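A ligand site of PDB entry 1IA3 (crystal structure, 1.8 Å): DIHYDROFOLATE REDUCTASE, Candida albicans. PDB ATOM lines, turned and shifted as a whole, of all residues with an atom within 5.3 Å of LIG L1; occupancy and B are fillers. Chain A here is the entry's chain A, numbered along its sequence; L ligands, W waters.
N of Ile 117 is in hydrogen-bond range of O1 of LIG L1 (3.2 Å).
O13 of LIG L1 lies within salt-bridge range of NH1 of Arg 79.
The side-chain hydroxyl (OG1) of Thr 58 sits at hydrogen-bond distance from an oxygen (O2) of LIG L1, at 2.6 Å.
N of Arg 56 is in hydrogen-bond range of O4 of LIG L1 (3.5 Å).
The backbone NH of Thr 58 is in hydrogen-bond range of an oxygen (O2) of LIG L1, 3.2 Å away.
The backbone NH of Glu 116 is in hydrogen-bond range of an oxygen (O9) of LIG L1, at 2.9 Å.
N of Ala 115 lies within hydrogen-bond range of O8 of LIG L1, at 3.0 Å.
O13 of LIG L1 is in hydrogen-bond range of N of Arg 79 (3.1 Å).
An oxygen (O12) of LIG L1 is in hydrogen-bond range of the side-chain hydroxyl (OG) of Ser 78.
The guanidinium group of Arg 56 is in salt-bridge range of an oxygen (O12) of LIG L1.
N of Gly 114 lies within hydrogen-bond range of O2 of LIG L1.
OG of Ser 78 sits close to N of Ser 80, 3.2 Å away.
O of Leu 77 sits at hydrogen-bond distance from N of Arg 56 (3.0 Å).
OG1 of Thr 58 sits at hydrogen-bond distance from N of Gly 114, at 3.1 Å.
N of Gly 55 lies within hydrogen-bond range of O of Gly 113.
The guanidinium group (NH2) of Arg 79 is in salt-bridge range of the side-chain carboxylate (OE1) of Glu 120, 3.3 Å away.
N of Leu 77 sits at hydrogen-bond distance from O of Met 54 (2.9 Å).
The side-chain carboxylate (OE1) of Glu 116 is in salt-bridge range of the guanidinium group (NH2) of Arg 79, 2.6 Å away.
Residues that only touch LIG L1: Gly 55, Lys 57, Leu 77, Ser 94, Gly 113 and Glu 120.
The nearest printed residue that does not touch LIG L1 is Gly 23 (4.1 Å).
Water W2 lies within hydrogen-bond range of the side-chain carboxylate (OE2) of Glu 116 and an oxygen (O5) of LIG L1.
Water W1 lies within hydrogen-bond range of NH1 of Arg 79 (2.7 Å) and O14 of LIG L1 (3.0 Å).
Water W4 lies within hydrogen-bond range of the side-chain amino group of Lys 57, the side-chain carboxylate of Glu 116 and an oxygen (O9) of LIG L1.
Water W6 lies within hydrogen-bond range of the side-chain hydroxyl (OG1) of Thr 58 (3.0 Å) and an oxygen (O8) of LIG L1 (3.3 Å).
Water W3 lies within hydrogen-bond range of NE of Arg 79 (2.8 Å) and N3 of LIG L1 (3.4 Å).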
ATOM      1  N   LYS A  22     -30.810   4.192  18.191  1.00  0.00           N
ATOM      2  CA  LYS A  22     -30.124   5.250  18.933  1.00  0.00           C
ATOM      3  C   LYS A  22     -30.383   5.171  20.416  1.00  0.00           C
ATOM      4  O   LYS A  22     -30.793   6.142  21.108  1.00  0.00           O
ATOM      5  CB  LYS A  22     -30.524   6.641  18.357  1.00  0.00           C
ATOM      6  N   GLY A  23     -30.172   3.953  20.951  1.00  0.00           N
ATOM      7  CA  GLY A  23     -30.262   3.668  22.364  1.00  0.00           C
ATOM      8  C   GLY A  23     -31.631   3.406  22.930  1.00  0.00           C
ATOM      9  O   GLY A  23     -31.681   3.132  24.161  1.00  0.00           O
ATOM     10  N   MET A  54     -27.018  -6.251  33.070  1.00  0.00           N
ATOM     11  CA  MET A  54     -27.090  -5.259  31.977  1.00  0.00           C
ATOM     12  C   MET A  54     -25.728  -4.654  31.727  1.00  0.00           C
ATOM     13  O   MET A  54     -24.912  -4.634  32.691  1.00  0.00           O
ATOM     14  CB  MET A  54     -28.194  -4.233  32.296  1.00  0.00           C
ATOM     15  CG  MET A  54     -27.766  -3.241  33.358  1.00  0.00           C
ATOM     16  SD  MET A  54     -29.200  -2.238  33.845  1.00  0.00           S
ATOM     17  CE  MET A  54     -29.779  -3.310  35.168  1.00  0.00           C
ATOM     18  N   GLY A  55     -25.534  -4.138  30.566  1.00  0.00           N
ATOM     19  CA  GLY A  55     -24.320  -3.393  30.155  1.00  0.00           C
ATOM     20  C   GLY A  55     -24.376  -1.985  30.736  1.00  0.00           C
ATOM     21  O   GLY A  55     -25.423  -1.409  31.086  1.00  0.00           O
ATOM     22  N   ARG A  56     -23.140  -1.420  30.907  1.00  0.00           N
ATOM     23  CA  ARG A  56     -23.061  -0.071  31.513  1.00  0.00           C
ATOM     24  C   ARG A  56     -23.878   0.938  30.709  1.00  0.00           C
ATOM     25  O   ARG A  56     -24.429   1.851  31.380  1.00  0.00           O
ATOM     26  CB  ARG A  56     -21.565   0.393  31.458  1.00  0.00           C
ATOM     27  CG  ARG A  56     -21.368   1.761  32.190  1.00  0.00           C
ATOM     28  CD  ARG A  56     -19.963   2.245  32.057  1.00  0.00           C
ATOM     29  NE  ARG A  56     -19.467   2.259  30.681  1.00  0.00           N
ATOM     30  CZ  ARG A  56     -19.678   3.027  29.661  1.00  0.00           C
ATOM     31  NH1 ARG A  56     -19.128   2.843  28.452  1.00  0.00           N
ATOM     32  NH2 ARG A  56     -20.420   4.144  29.735  1.00  0.00           N
ATOM     33  N   LYS A  57     -23.897   0.885  29.421  1.00  0.00           N
ATOM     34  CA  LYS A  57     -24.654   1.925  28.638  1.00  0.00           C
ATOM     35  C   LYS A  57     -26.156   1.853  28.917  1.00  0.00           C
ATOM     36  O   LYS A  57     -26.810   2.934  29.008  1.00  0.00           O
ATOM     37  CB  LYS A  57     -24.354   1.841  27.168  1.00  0.00           C
ATOM     38  CG  LYS A  57     -22.921   2.220  26.817  1.00  0.00           C
ATOM     39  CD  LYS A  57     -22.641   1.945  25.361  1.00  0.00           C
ATOM     40  CE  LYS A  57     -21.180   1.977  24.973  1.00  0.00           C
ATOM     41  NZ  LYS A  57     -21.053   1.477  23.530  1.00  0.00           N
ATOM     42  N   THR A  58     -26.705   0.671  29.038  1.00  0.00           N
ATOM     43  CA  THR A  58     -28.123   0.460  29.413  1.00  0.00           C
ATOM     44  C   THR A  58     -28.379   1.058  30.783  1.00  0.00           C
ATOM     45  O   THR A  58     -29.326   1.820  30.938  1.00  0.00           O
ATOM     46  CB  THR A  58     -28.581  -1.053  29.289  1.00  0.00           C
ATOM     47  OG1 THR A  58     -28.491  -1.295  27.832  1.00  0.00           O
ATOM     48  CG2 THR A  58     -30.057  -1.253  29.746  1.00  0.00           C
ATOM     49  N   LEU A  77     -22.305  -4.645  34.036  1.00  0.00           N
ATOM     50  CA  LEU A  77     -20.991  -5.031  33.525  1.00  0.00           C
ATOM     51  C   LEU A  77     -20.316  -3.876  32.764  1.00  0.00           C
ATOM     52  O   LEU A  77     -20.922  -3.263  31.897  1.00  0.00           O
ATOM     53  CB  LEU A  77     -21.141  -6.255  32.597  1.00  0.00           C
ATOM     54  CG  LEU A  77     -21.862  -7.479  33.184  1.00  0.00           C
ATOM     55  CD1 LEU A  77     -21.980  -8.508  32.026  1.00  0.00           C
ATOM     56  CD2 LEU A  77     -21.071  -8.075  34.316  1.00  0.00           C
ATOM     57  N   SER A  78     -19.004  -3.817  33.051  1.00  0.00           N
ATOM     58  CA  SER A  78     -18.147  -2.843  32.300  1.00  0.00           C
ATOM     59  C   SER A  78     -16.753  -3.515  32.347  1.00  0.00           C
ATOM     60  O   SER A  78     -16.443  -4.143  33.344  1.00  0.00           O
ATOM     61  CB  SER A  78     -18.133  -1.476  32.960  1.00  0.00           C
ATOM     62  OG  SER A  78     -17.058  -0.683  32.449  1.00  0.00           O
ATOM     63  N   ARG A  79     -16.040  -3.395  31.253  1.00  0.00           N
ATOM     64  CA  ARG A  79     -14.650  -3.929  31.199  1.00  0.00           C
ATOM     65  C   ARG A  79     -13.717  -3.180  32.134  1.00  0.00           C
ATOM     66  O   ARG A  79     -12.642  -3.688  32.516  1.00  0.00           O
ATOM     67  CB  ARG A  79     -14.205  -3.922  29.728  1.00  0.00           C
ATOM     68  CG  ARG A  79     -14.969  -4.996  28.967  1.00  0.00           C
ATOM     69  CD  ARG A  79     -14.498  -5.103  27.584  1.00  0.00           C
ATOM     70  NE  ARG A  79     -15.423  -5.579  26.593  1.00  0.00           N
ATOM     71  CZ  ARG A  79     -16.340  -4.863  25.947  1.00  0.00           C
ATOM     72  NH1 ARG A  79     -16.474  -3.542  26.078  1.00  0.00           N
ATOM     73  NH2 ARG A  79     -17.205  -5.538  25.160  1.00  0.00           N
ATOM     74  N   SER A  80     -14.118  -1.981  32.549  1.00  0.00           N
ATOM     75  CA  SER A  80     -13.377  -1.098  33.455  1.00  0.00           C
ATOM     76  C   SER A  80     -13.730  -1.314  34.912  1.00  0.00           C
ATOM     77  O   SER A  80     -13.134  -0.700  35.837  1.00  0.00           O
ATOM     78  CB  SER A  80     -13.547   0.358  33.116  1.00  0.00           C
ATOM     79  OG  SER A  80     -13.087   0.770  31.875  1.00  0.00           O
ATOM     80  N   SER A  94     -16.784  -7.191  35.867  1.00  0.00           N
ATOM     81  CA  SER A  94     -16.257  -7.124  34.507  1.00  0.00           C
ATOM     82  C   SER A  94     -16.619  -8.344  33.679  1.00  0.00           C
ATOM     83  O   SER A  94     -16.216  -8.387  32.499  1.00  0.00           O
ATOM     84  CB  SER A  94     -14.771  -6.838  34.375  1.00  0.00           C
ATOM     85  OG  SER A  94     -14.086  -7.886  35.075  1.00  0.00           O
ATOM     86  N   SER A  95     -17.234  -9.368  34.301  1.00  0.00           N
ATOM     87  CA  SER A  95     -17.670 -10.528  33.536  1.00  0.00           C
ATOM     88  C   SER A  95     -18.910 -11.133  34.259  1.00  0.00           C
ATOM     89  O   SER A  95     -19.039 -10.972  35.468  1.00  0.00           O
ATOM     90  CB  SER A  95     -16.659 -11.622  33.301  1.00  0.00           C
ATOM     91  OG  SER A  95     -16.378 -12.360  34.438  1.00  0.00           O
ATOM     92  N   GLY A 113     -29.966  -6.698  28.519  1.00  0.00           N
ATOM     93  CA  GLY A 113     -29.506  -5.858  27.467  1.00  0.00           C
ATOM     94  C   GLY A 113     -28.235  -5.106  27.865  1.00  0.00           C
ATOM     95  O   GLY A 113     -27.764  -5.334  28.940  1.00  0.00           O
ATOM     96  N   GLY A 114     -27.740  -4.229  26.972  1.00  0.00           N
ATOM     97  CA  GLY A 114     -28.358  -3.983  25.673  1.00  0.00           C
ATOM     98  C   GLY A 114     -27.775  -4.796  24.547  1.00  0.00           C
ATOM     99  O   GLY A 114     -27.414  -5.973  24.722  1.00  0.00           O
ATOM    100  N   ALA A 115     -27.663  -4.137  23.372  1.00  0.00           N
ATOM    101  CA  ALA A 115     -27.271  -4.808  22.118  1.00  0.00           C
ATOM    102  C   ALA A 115     -25.961  -5.543  22.163  1.00  0.00           C
ATOM    103  O   ALA A 115     -25.854  -6.727  21.776  1.00  0.00           O
ATOM    104  CB  ALA A 115     -27.368  -3.863  20.945  1.00  0.00           C
ATOM    105  N   GLU A 116     -24.928  -4.878  22.683  1.00  0.00           N
ATOM    106  CA  GLU A 116     -23.608  -5.495  22.785  1.00  0.00           C
ATOM    107  C   GLU A 116     -23.638  -6.654  23.728  1.00  0.00           C
ATOM    108  O   GLU A 116     -23.086  -7.725  23.372  1.00  0.00           O
ATOM    109  CB  GLU A 116     -22.513  -4.480  23.061  1.00  0.00           C
ATOM    110  CG  GLU A 116     -21.110  -5.073  23.047  1.00  0.00           C
ATOM    111  CD  GLU A 116     -19.990  -4.134  23.338  1.00  0.00           C
ATOM    112  OE1 GLU A 116     -18.835  -4.557  23.362  1.00  0.00           O
ATOM    113  OE2 GLU A 116     -20.254  -2.951  23.584  1.00  0.00           O
ATOM    114  N   ILE A 117     -24.243  -6.491  24.875  1.00  0.00           N
ATOM    115  CA  ILE A 117     -24.357  -7.609  25.869  1.00  0.00           C
ATOM    116  C   ILE A 117     -25.033  -8.807  25.265  1.00  0.00           C
ATOM    117  O   ILE A 117     -24.622  -9.979  25.344  1.00  0.00           O
ATOM    118  CB  ILE A 117     -25.135  -7.016  27.120  1.00  0.00           C
ATOM    119  CG1 ILE A 117     -24.226  -5.992  27.829  1.00  0.00           C
ATOM    120  CG2 ILE A 117     -25.658  -8.137  28.073  1.00  0.00           C
ATOM    121  CD1 ILE A 117     -22.987  -6.515  28.554  1.00  0.00           C
ATOM    122  N   GLU A 120     -22.900 -10.643  22.531  1.00  0.00           N
ATOM    123  CA  GLU A 120     -21.700 -11.288  23.094  1.00  0.00           C
ATOM    124  C   GLU A 120     -22.058 -12.479  23.985  1.00  0.00           C
ATOM    125  O   GLU A 120     -21.430 -13.540  23.867  1.00  0.00           O
ATOM    126  CB  GLU A 120     -21.003 -10.268  24.003  1.00  0.00           C
ATOM    127  CG  GLU A 120     -19.520 -10.264  24.064  1.00  0.00           C
ATOM    128  CD  GLU A 120     -18.877  -9.224  23.172  1.00  0.00           C
ATOM    129  OE1 GLU A 120     -18.245  -8.325  23.691  1.00  0.00           O
ATOM    130  OE2 GLU A 120     -19.052  -9.449  21.959  1.00  0.00           O
ATOM    131  N   LEU A 121     -23.033 -12.375  24.881  1.00  0.00           N
ATOM    132  CA  LEU A 121     -23.409 -13.383  25.832  1.00  0.00           C
ATOM    133  C   LEU A 121     -24.245 -14.516  25.341  1.00  0.00           C
ATOM    134  O   LEU A 121     -24.272 -15.596  25.995  1.00  0.00           O
ATOM    135  CB  LEU A 121     -23.916 -12.725  27.121  1.00  0.00           C
ATOM    136  CG  LEU A 121     -22.965 -11.738  27.798  1.00  0.00           C
ATOM    137  CD1 LEU A 121     -23.711 -10.998  28.910  1.00  0.00           C
ATOM    138  CD2 LEU A 121     -21.786 -12.516  28.409  1.00  0.00           C
ATOM    139  N   THR A 147     -29.921  -1.267  15.580  1.00  0.00           N
ATOM    140  CA  THR A 147     -29.341  -2.433  16.263  1.00  0.00           C
ATOM    141  C   THR A 147     -30.220  -3.648  16.048  1.00  0.00           C
ATOM    142  O   THR A 147     -31.431  -3.551  15.931  1.00  0.00           O
ATOM    143  CB  THR A 147     -28.996  -2.247  17.765  1.00  0.00           C
ATOM    144  OG1 THR A 147     -30.232  -1.828  18.415  1.00  0.00           O
ATOM    145  CG2 THR A 147     -27.865  -1.239  18.072  1.00  0.00           C
HETATM  146  P1  LIG L   1     -25.025  -2.171  26.344  1.00  0.00           P
HETATM  147  O1  LIG L   1     -24.939  -3.443  25.738  1.00  0.00           O
HETATM  148  O2  LIG L   1     -26.027  -1.930  27.376  1.00  0.00           O
HETATM  149  O3  LIG L   1     -23.617  -1.726  27.033  1.00  0.00           O
HETATM  150  C1  LIG L   1     -22.396  -2.017  26.299  1.00  0.00           C
HETATM  151  C2  LIG L   1     -21.302  -1.825  27.377  1.00  0.00           C
HETATM  152  O4  LIG L   1     -21.368  -2.921  28.301  1.00  0.00           O
HETATM  153  C3  LIG L   1     -19.872  -1.900  26.759  1.00  0.00           C
HETATM  154  O5  LIG L   1     -19.573  -0.553  26.311  1.00  0.00           O
HETATM  155  C4  LIG L   1     -19.091  -2.364  28.043  1.00  0.00           C
HETATM  156  O6  LIG L   1     -19.012  -1.358  29.082  1.00  0.00           O
HETATM  157  C5  LIG L   1     -20.104  -3.359  28.640  1.00  0.00           C
HETATM  158  N1  LIG L   1     -19.857  -4.659  28.112  1.00  0.00           N
HETATM  159  C6  LIG L   1     -20.310  -5.061  26.871  1.00  0.00           C
HETATM  160  N2  LIG L   1     -19.968  -6.322  26.610  1.00  0.00           N
HETATM  161  C7  LIG L   1     -19.299  -6.694  27.756  1.00  0.00           C
HETATM  162  C8  LIG L   1     -18.678  -7.927  28.021  1.00  0.00           C
HETATM  163  N3  LIG L   1     -18.753  -8.944  27.132  1.00  0.00           N
HETATM  164  N4  LIG L   1     -18.063  -8.015  29.230  1.00  0.00           N
HETATM  165  C9  LIG L   1     -18.059  -6.923  30.054  1.00  0.00           C
HETATM  166  N5  LIG L   1     -18.560  -5.734  29.873  1.00  0.00           N
HETATM  167  C10 LIG L   1     -19.208  -5.697  28.671  1.00  0.00           C
HETATM  168  O7  LIG L   1     -25.183  -1.009  25.278  1.00  0.00           O
HETATM  169  P2  LIG L   1     -25.584  -1.008  23.724  1.00  0.00           P
HETATM  170  O8  LIG L   1     -27.078  -1.237  23.664  1.00  0.00           O
HETATM  171  O9  LIG L   1     -24.818  -1.953  22.911  1.00  0.00           O
HETATM  172  O10 LIG L   1     -25.269   0.482  23.281  1.00  0.00           O
HETATM  173  C11 LIG L   1     -26.252   1.518  23.317  1.00  0.00           C
HETATM  174  C12 LIG L   1     -25.672   2.706  22.516  1.00  0.00           C
HETATM  175  O11 LIG L   1     -25.748   2.417  21.088  1.00  0.00           O
HETATM  176  C13 LIG L   1     -26.237   4.047  22.827  1.00  0.00           C
HETATM  177  P3  LIG L   1     -17.599  -0.521  29.020  1.00  0.00           P
HETATM  178  O12 LIG L   1     -17.726   0.310  30.311  1.00  0.00           O
HETATM  179  O13 LIG L   1     -16.554  -1.502  28.894  1.00  0.00           O
HETATM  180  O14 LIG L   1     -17.706   0.325  27.803  1.00  0.00           O
HETATM  181  C1  LG2 L   2     -38.326  -5.229  27.772  1.00  0.00           C
HETATM  182  C2  LG2 L   2     -36.937  -5.251  28.057  1.00  0.00           C
HETATM  183  C3  LG2 L   2     -36.270  -6.558  27.742  1.00  0.00           C
HETATM  184  N1  LG2 L   2     -36.888  -7.550  27.249  1.00  0.00           N
HETATM  185  C4  LG2 L   2     -38.229  -7.569  27.077  1.00  0.00           C
HETATM  186  N2  LG2 L   2     -38.951  -6.374  27.186  1.00  0.00           N
HETATM  187  N3  LG2 L   2     -34.982  -6.828  28.012  1.00  0.00           N
HETATM  188  C5  LG2 L   2     -39.076  -4.070  28.044  1.00  0.00           C
HETATM  189  C6  LG2 L   2     -38.482  -2.946  28.535  1.00  0.00           C
HETATM  190  C7  LG2 L   2     -37.125  -2.923  28.848  1.00  0.00           C
HETATM  191  C8  LG2 L   2     -36.355  -4.097  28.575  1.00  0.00           C
HETATM  192  N4  LG2 L   2     -38.834  -8.608  26.531  1.00  0.00           N
HETATM  193  S1  LG2 L   2     -34.656  -3.943  29.043  1.00  0.00           S
HETATM  194  C9  LG2 L   2     -33.904  -3.400  27.478  1.00  0.00           C
HETATM  195  C10 LG2 L   2     -34.419  -3.500  26.195  1.00  0.00           C
HETATM  196  C11 LG2 L   2     -33.805  -3.138  24.997  1.00  0.00           C
HETATM  197  C12 LG2 L   2     -32.482  -2.502  25.034  1.00  0.00           C
HETATM  198  C13 LG2 L   2     -31.976  -2.439  26.293  1.00  0.00           C
HETATM  199  C14 LG2 L   2     -32.611  -2.823  27.491  1.00  0.00           C
HETATM  200  C15 LG2 L   2     -31.891  -1.948  23.759  1.00  0.00           C
HETATM  201  C16 LG2 L   2     -30.410  -1.533  23.735  1.00  0.00           C
HETATM  202  C17 LG2 L   2     -32.133  -2.955  22.649  1.00  0.00           C
HETATM  203  C18 LG2 L   2     -32.581  -0.554  23.361  1.00  0.00           C
HETATM  204  O   HOH W   1     -15.787  -0.944  25.928  1.00  0.00           O
HETATM  205  O   HOH W   2     -18.366  -1.163  23.924  1.00  0.00           O
HETATM  206  O   HOH W   3     -15.609  -8.337  26.109  1.00  0.00           O
HETATM  207  O   HOH W   4     -21.983  -0.934  22.899  1.00  0.00           O
HETATM  208  O   HOH W   5     -16.721 -11.257  27.291  1.00  0.00           O
HETATM  209  O   HOH W   6     -28.510   0.880  25.782  1.00  0.00           O
HETATM  210  O   HOH W   7     -15.932   2.342  30.214  1.00  0.00           O
HETATM  211  O   HOH W   8     -24.312  -2.187  19.981  1.00  0.00           O
